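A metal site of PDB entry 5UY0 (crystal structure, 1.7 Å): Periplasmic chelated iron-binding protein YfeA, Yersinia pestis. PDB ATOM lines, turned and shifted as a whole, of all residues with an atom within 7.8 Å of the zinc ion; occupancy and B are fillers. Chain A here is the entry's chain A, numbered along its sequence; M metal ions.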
ATOM      1  N   GLU A  74      13.499   6.904   7.164  1.00  0.00           N
ATOM      2  CA  GLU A  74      13.152   7.463   8.473  1.00  0.00           C
ATOM      3  C   GLU A  74      11.917   6.758   9.028  1.00  0.00           C
ATOM      4  O   GLU A  74      10.891   6.660   8.355  1.00  0.00           O
ATOM      5  CB  GLU A  74      12.917   8.966   8.324  1.00  0.00           C
ATOM      6  CG  GLU A  74      13.123   9.777   9.564  1.00  0.00           C
ATOM      7  CD  GLU A  74      12.044   9.516  10.564  1.00  0.00           C
ATOM      8  OE1 GLU A  74      10.866   9.719  10.219  1.00  0.00           O
ATOM      9  OE2 GLU A  74      12.381   9.071  11.692  1.00  0.00           O
ATOM     10  N   ILE A  75      12.015   6.247  10.261  1.00  0.00           N
ATOM     11  CA  ILE A  75      11.020   5.316  10.770  1.00  0.00           C
ATOM     12  C   ILE A  75       9.956   5.966  11.657  1.00  0.00           C
ATOM     13  O   ILE A  75       8.863   5.396  11.796  1.00  0.00           O
ATOM     14  CB  ILE A  75      11.694   4.157  11.555  1.00  0.00           C
ATOM     15  CG1 ILE A  75      12.449   4.709  12.756  1.00  0.00           C
ATOM     16  CG2 ILE A  75      12.666   3.387  10.654  1.00  0.00           C
ATOM     17  CD1 ILE A  75      13.078   3.589  13.626  1.00  0.00           C
ATOM     18  N   HIS A  76      10.243   7.111  12.279  1.00  0.00           N
ATOM     19  CA  HIS A  76       9.300   7.677  13.239  1.00  0.00           C
ATOM     20  C   HIS A  76       8.045   8.171  12.543  1.00  0.00           C
ATOM     21  O   HIS A  76       6.926   7.921  13.006  1.00  0.00           O
ATOM     22  CB  HIS A  76       9.930   8.840  14.010  1.00  0.00           C
ATOM     23  CG  HIS A  76      11.125   8.465  14.839  1.00  0.00           C
ATOM     24  ND1 HIS A  76      11.085   8.432  16.217  1.00  0.00           N
ATOM     25  CD2 HIS A  76      12.388   8.139  14.484  1.00  0.00           C
ATOM     26  CE1 HIS A  76      12.270   8.086  16.679  1.00  0.00           C
ATOM     27  NE2 HIS A  76      13.083   7.912  15.648  1.00  0.00           N
ATOM     28  N   LEU A 101       7.332   4.658  19.088  1.00  0.00           N
ATOM     29  CA  LEU A 101       8.361   4.879  18.065  1.00  0.00           C
ATOM     30  C   LEU A 101       7.718   5.157  16.713  1.00  0.00           C
ATOM     31  O   LEU A 101       8.020   6.164  16.047  1.00  0.00           O
ATOM     32  CB  LEU A 101       9.265   3.651  17.936  1.00  0.00           C
ATOM     33  CG  LEU A 101      10.245   3.727  16.753  1.00  0.00           C
ATOM     34  CD1 LEU A 101      11.305   4.806  16.933  1.00  0.00           C
ATOM     35  CD2 LEU A 101      10.895   2.370  16.497  1.00  0.00           C
ATOM     36  N   ASN A 139      11.471   7.797  25.490  1.00  0.00           N
ATOM     37  CA  ASN A 139      12.468   7.711  24.438  1.00  0.00           C
ATOM     38  C   ASN A 139      12.391   6.300  23.873  1.00  0.00           C
ATOM     39  O   ASN A 139      12.575   5.341  24.614  1.00  0.00           O
ATOM     40  CB  ASN A 139      13.864   8.008  25.005  1.00  0.00           C
ATOM     41  CG  ASN A 139      14.958   8.004  23.944  1.00  0.00           C
ATOM     42  OD1 ASN A 139      14.899   7.245  22.977  1.00  0.00           O
ATOM     43  ND2 ASN A 139      15.965   8.847  24.143  1.00  0.00           N
ATOM     44  N   PRO A 140      12.052   6.128  22.593  1.00  0.00           N
ATOM     45  CA  PRO A 140      11.751   4.781  22.093  1.00  0.00           C
ATOM     46  C   PRO A 140      12.977   3.965  21.731  1.00  0.00           C
ATOM     47  O   PRO A 140      12.834   2.780  21.428  1.00  0.00           O
ATOM     48  CB  PRO A 140      10.926   5.086  20.824  1.00  0.00           C
ATOM     49  CG  PRO A 140      11.559   6.361  20.320  1.00  0.00           C
ATOM     50  CD  PRO A 140      11.952   7.153  21.544  1.00  0.00           C
ATOM     51  N   HIS A 141      14.167   4.570  21.749  1.00  0.00           N
ATOM     52  CA  HIS A 141      15.348   3.921  21.180  1.00  0.00           C
ATOM     53  C   HIS A 141      15.976   2.906  22.143  1.00  0.00           C
ATOM     54  O   HIS A 141      17.200   2.908  22.331  1.00  0.00           O
ATOM     55  CB  HIS A 141      16.378   4.982  20.779  1.00  0.00           C
ATOM     56  CG  HIS A 141      15.864   5.987  19.776  1.00  0.00           C
ATOM     57  ND1 HIS A 141      15.415   7.247  20.146  1.00  0.00           N
ATOM     58  CD2 HIS A 141      15.766   5.938  18.425  1.00  0.00           C
ATOM     59  CE1 HIS A 141      15.060   7.923  19.061  1.00  0.00           C
ATOM     60  NE2 HIS A 141      15.264   7.147  18.003  1.00  0.00           N
ATOM     61  N   TRP A 143      16.605  -0.209  22.059  1.00  0.00           N
ATOM     62  CA  TRP A 143      17.478  -1.268  21.539  1.00  0.00           C
ATOM     63  C   TRP A 143      18.939  -0.872  21.502  1.00  0.00           C
ATOM     64  O   TRP A 143      19.789  -1.731  21.210  1.00  0.00           O
ATOM     65  CB  TRP A 143      17.051  -1.668  20.116  1.00  0.00           C
ATOM     66  CG  TRP A 143      17.169  -0.528  19.126  1.00  0.00           C
ATOM     67  CD1 TRP A 143      18.267  -0.196  18.381  1.00  0.00           C
ATOM     68  CD2 TRP A 143      16.150   0.419  18.778  1.00  0.00           C
ATOM     69  NE1 TRP A 143      17.990   0.912  17.594  1.00  0.00           N
ATOM     70  CE2 TRP A 143      16.691   1.306  17.815  1.00  0.00           C
ATOM     71  CE3 TRP A 143      14.812   0.602  19.174  1.00  0.00           C
ATOM     72  CZ2 TRP A 143      15.965   2.356  17.258  1.00  0.00           C
ATOM     73  CZ3 TRP A 143      14.085   1.642  18.626  1.00  0.00           C
ATOM     74  CH2 TRP A 143      14.669   2.515  17.686  1.00  0.00           C
ATOM     75  N   GLU A 207      19.900  13.448  16.371  1.00  0.00           N
ATOM     76  CA  GLU A 207      18.790  12.983  17.189  1.00  0.00           C
ATOM     77  C   GLU A 207      19.304  12.515  18.537  1.00  0.00           C
ATOM     78  O   GLU A 207      20.383  11.917  18.624  1.00  0.00           O
ATOM     79  CB  GLU A 207      18.021  11.834  16.501  1.00  0.00           C
ATOM     80  CG  GLU A 207      16.727  11.444  17.259  1.00  0.00           C
ATOM     81  CD  GLU A 207      15.962  10.258  16.684  1.00  0.00           C
ATOM     82  OE1 GLU A 207      16.540   9.375  16.009  1.00  0.00           O
ATOM     83  OE2 GLU A 207      14.738  10.187  16.957  1.00  0.00           O
ATOM     84  N   GLY A 208      18.528  12.771  19.594  1.00  0.00           N
ATOM     85  CA  GLY A 208      18.887  12.279  20.923  1.00  0.00           C
ATOM     86  C   GLY A 208      18.530  10.815  21.064  1.00  0.00           C
ATOM     87  O   GLY A 208      17.821  10.413  21.996  1.00  0.00           O
ATOM     88  N   ALA A 209      19.036   9.998  20.146  1.00  0.00           N
ATOM     89  CA  ALA A 209      18.605   8.612  20.004  1.00  0.00           C
ATOM     90  C   ALA A 209      19.479   7.648  20.776  1.00  0.00           C
ATOM     91  O   ALA A 209      19.253   6.432  20.701  1.00  0.00           O
ATOM     92  CB  ALA A 209      18.597   8.207  18.526  1.00  0.00           C
ATOM     93  N   PHE A 210      20.465   8.143  21.532  1.00  0.00           N
ATOM     94  CA  PHE A 210      21.475   7.272  22.125  1.00  0.00           C
ATOM     95  C   PHE A 210      21.398   7.239  23.641  1.00  0.00           C
ATOM     96  O   PHE A 210      22.309   6.718  24.286  1.00  0.00           O
ATOM     97  CB  PHE A 210      22.863   7.711  21.641  1.00  0.00           C
ATOM     98  CG  PHE A 210      22.994   7.642  20.166  1.00  0.00           C
ATOM     99  CD1 PHE A 210      23.356   6.457  19.541  1.00  0.00           C
ATOM    100  CD2 PHE A 210      22.651   8.743  19.384  1.00  0.00           C
ATOM    101  CE1 PHE A 210      23.432   6.386  18.155  1.00  0.00           C
ATOM    102  CE2 PHE A 210      22.727   8.672  17.998  1.00  0.00           C
ATOM    103  CZ  PHE A 210      23.122   7.491  17.382  1.00  0.00           C
ATOM    104  N   TRP A 225      18.283  17.636  18.374  1.00  0.00           N
ATOM    105  CA  TRP A 225      16.845  17.564  18.615  1.00  0.00           C
ATOM    106  C   TRP A 225      16.556  16.293  19.398  1.00  0.00           C
ATOM    107  O   TRP A 225      17.236  15.292  19.208  1.00  0.00           O
ATOM    108  CB  TRP A 225      16.016  17.591  17.311  1.00  0.00           C
ATOM    109  CG  TRP A 225      16.384  16.542  16.283  1.00  0.00           C
ATOM    110  CD1 TRP A 225      15.881  15.281  16.179  1.00  0.00           C
ATOM    111  CD2 TRP A 225      17.292  16.708  15.197  1.00  0.00           C
ATOM    112  NE1 TRP A 225      16.450  14.636  15.100  1.00  0.00           N
ATOM    113  CE2 TRP A 225      17.321  15.489  14.480  1.00  0.00           C
ATOM    114  CE3 TRP A 225      18.117  17.764  14.758  1.00  0.00           C
ATOM    115  CZ2 TRP A 225      18.127  15.308  13.351  1.00  0.00           C
ATOM    116  CZ3 TRP A 225      18.908  17.568  13.643  1.00  0.00           C
ATOM    117  CH2 TRP A 225      18.905  16.357  12.952  1.00  0.00           C
ATOM    118  N   PRO A 226      15.565  16.316  20.276  1.00  0.00           N
ATOM    119  CA  PRO A 226      15.416  15.195  21.217  1.00  0.00           C
ATOM    120  C   PRO A 226      14.861  13.941  20.558  1.00  0.00           C
ATOM    121  O   PRO A 226      15.252  12.834  20.952  1.00  0.00           O
ATOM    122  CB  PRO A 226      14.478  15.746  22.294  1.00  0.00           C
ATOM    123  CG  PRO A 226      13.853  16.981  21.696  1.00  0.00           C
ATOM    124  CD  PRO A 226      14.779  17.509  20.671  1.00  0.00           C
ATOM    125  N   ILE A 227      13.976  14.073  19.572  1.00  0.00           N
ATOM    126  CA  ILE A 227      13.426  12.932  18.850  1.00  0.00           C
ATOM    127  C   ILE A 227      13.018  13.419  17.462  1.00  0.00           C
ATOM    128  O   ILE A 227      12.579  14.555  17.296  1.00  0.00           O
ATOM    129  CB  ILE A 227      12.246  12.288  19.619  1.00  0.00           C
ATOM    130  CG1 ILE A 227      11.774  11.008  18.930  1.00  0.00           C
ATOM    131  CG2 ILE A 227      11.083  13.275  19.820  1.00  0.00           C
ATOM    132  CD1 ILE A 227      10.830  10.152  19.792  1.00  0.00           C
ATOM    133  N   ASN A 228      13.210  12.545  16.463  1.00  0.00           N
ATOM    134  CA  ASN A 228      12.832  12.909  15.098  1.00  0.00           C
ATOM    135  C   ASN A 228      11.358  13.301  15.058  1.00  0.00           C
ATOM    136  O   ASN A 228      10.509  12.633  15.638  1.00  0.00           O
ATOM    137  CB  ASN A 228      13.054  11.737  14.123  1.00  0.00           C
ATOM    138  CG  ASN A 228      14.504  11.440  13.884  1.00  0.00           C
ATOM    139  OD1 ASN A 228      15.403  12.115  14.388  1.00  0.00           O
ATOM    140  ND2 ASN A 228      14.754  10.381  13.114  1.00  0.00           N
ATOM    141  N   GLU A 256      23.315  10.804  12.140  1.00  0.00           N
ATOM    142  CA  GLU A 256      22.792   9.450  12.077  1.00  0.00           C
ATOM    143  C   GLU A 256      22.317   9.127  10.671  1.00  0.00           C
ATOM    144  O   GLU A 256      22.034  10.017   9.854  1.00  0.00           O
ATOM    145  CB  GLU A 256      21.649   9.239  13.072  1.00  0.00           C
ATOM    146  CG  GLU A 256      22.073   9.512  14.509  1.00  0.00           C
ATOM    147  CD  GLU A 256      21.827  10.953  14.906  1.00  0.00           C
ATOM    148  OE1 GLU A 256      20.692  11.422  14.720  1.00  0.00           O
ATOM    149  OE2 GLU A 256      22.768  11.603  15.396  1.00  0.00           O
ATOM    150  N   THR A 258      19.646   7.937   9.125  1.00  0.00           N
ATOM    151  CA  THR A 258      18.372   8.209   8.470  1.00  0.00           C
ATOM    152  C   THR A 258      17.997   9.680   8.450  1.00  0.00           C
ATOM    153  O   THR A 258      16.872  10.014   8.038  1.00  0.00           O
ATOM    154  CB  THR A 258      17.228   7.414   9.120  1.00  0.00           C
ATOM    155  OG1 THR A 258      16.953   7.954  10.416  1.00  0.00           O
ATOM    156  CG2 THR A 258      17.578   5.946   9.230  1.00  0.00           C
ATOM    157  N   ILE A 259      18.901  10.573   8.872  1.00  0.00           N
ATOM    158  CA  ILE A 259      18.614  11.992   8.924  1.00  0.00           C
ATOM    159  C   ILE A 259      19.770  12.755   8.284  1.00  0.00           C
ATOM    160  O   ILE A 259      20.813  12.201   7.941  1.00  0.00           O
ATOM    161  CB  ILE A 259      18.332  12.489  10.368  1.00  0.00           C
ATOM    162  CG1 ILE A 259      19.382  11.979  11.358  1.00  0.00           C
ATOM    163  CG2 ILE A 259      16.957  12.019  10.839  1.00  0.00           C
ATOM    164  CD1 ILE A 259      20.654  12.861  11.433  1.00  0.00           C
ATOM    165  N   VAL A 281      21.400   3.982  14.224  1.00  0.00           N
ATOM    166  CA  VAL A 281      20.482   3.730  15.337  1.00  0.00           C
ATOM    167  C   VAL A 281      19.090   3.303  14.824  1.00  0.00           C
ATOM    168  O   VAL A 281      18.562   2.279  15.247  1.00  0.00           O
ATOM    169  CB  VAL A 281      20.369   4.952  16.290  1.00  0.00           C
ATOM    170  CG1 VAL A 281      20.054   6.259  15.547  1.00  0.00           C
ATOM    171  CG2 VAL A 281      19.327   4.703  17.411  1.00  0.00           C
ATOM    172  N   ASP A 282      18.511   4.079  13.925  1.00  0.00           N
ATOM    173  CA  ASP A 282      17.147   3.811  13.474  1.00  0.00           C
ATOM    174  C   ASP A 282      17.063   2.857  12.303  1.00  0.00           C
ATOM    175  O   ASP A 282      15.955   2.470  11.926  1.00  0.00           O
ATOM    176  CB  ASP A 282      16.450   5.113  13.068  1.00  0.00           C
ATOM    177  CG  ASP A 282      16.066   5.973  14.245  1.00  0.00           C
ATOM    178  OD1 ASP A 282      16.215   5.502  15.390  1.00  0.00           O
ATOM    179  OD2 ASP A 282      15.612   7.118  14.021  1.00  0.00           O
ATOM    180  N   SER A 283      18.180   2.491  11.687  1.00  0.00           N
ATOM    181  CA  SER A 283      18.083   1.603  10.538  1.00  0.00           C
ATOM    182  C   SER A 283      19.390   0.867  10.350  1.00  0.00           C
ATOM    183  O   SER A 283      20.471   1.398  10.641  1.00  0.00           O
ATOM    184  CB  SER A 283      17.754   2.380   9.256  1.00  0.00           C
ATOM    185  OG  SER A 283      17.682   1.466   8.179  1.00  0.00           O
HETATM  186 ZN    ZN M   1      15.141   7.847  16.026  1.00  0.00          ZN
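The side-chain carboxylate (OE1) of Glu 207 binds the zinc ion, 2.1 Å away.
The zinc ion is bound by NE2 of His 76 (2.1 Å).
The zinc ion is bound by NE2 of His 141, 2.1 Å away.
OD2 of Asp 282 is bound to the zinc ion, at 2.2 Å.
The side-chain carboxylate (OE2) of Glu 207 binds the zinc ion (2.6 Å).
The zinc ion has five donor atoms within binding distance.
Slightly farther from the zinc ion lies OD1 of Asp 282 (2.7 Å).
OE2 of Glu 207 sits close to N of Asn 228.
The side-chain carboxylate of Glu 256 sits at hydrogen-bond distance from the backbone NH of Glu 207 (2.7 Å).
N of His 76 lies close to OE2 of Glu 74 (3.0 Å).
A ring nitrogen (ND1) of His 141 lies within hydrogen-bond range of the side-chain amide oxygen of Asn 139, at 2.9 Å.
The side-chain amide nitrogen (ND2) of Asn 228 lies close to the side-chain carboxylate (OD2) of Asp 282 (3.5 Å).
ND2 of Asn 228 is in hydrogen-bond range of OE2 of Glu 74 (3.1 Å).
The side-chain amide oxygen of Asn 228 sits at hydrogen-bond distance from the indole nitrogen of Trp 225 (2.8 Å).
ND2 of Asn 228 touches the zinc ion, at 3.9 Å.
Five residues have an atom within 4 Å of the zinc ion: His 76, His 141, Glu 207, Asn 228 and Asp 282.
The nearest printed residue that does not touch the zinc ion is Ala 209 (4.3 Å).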
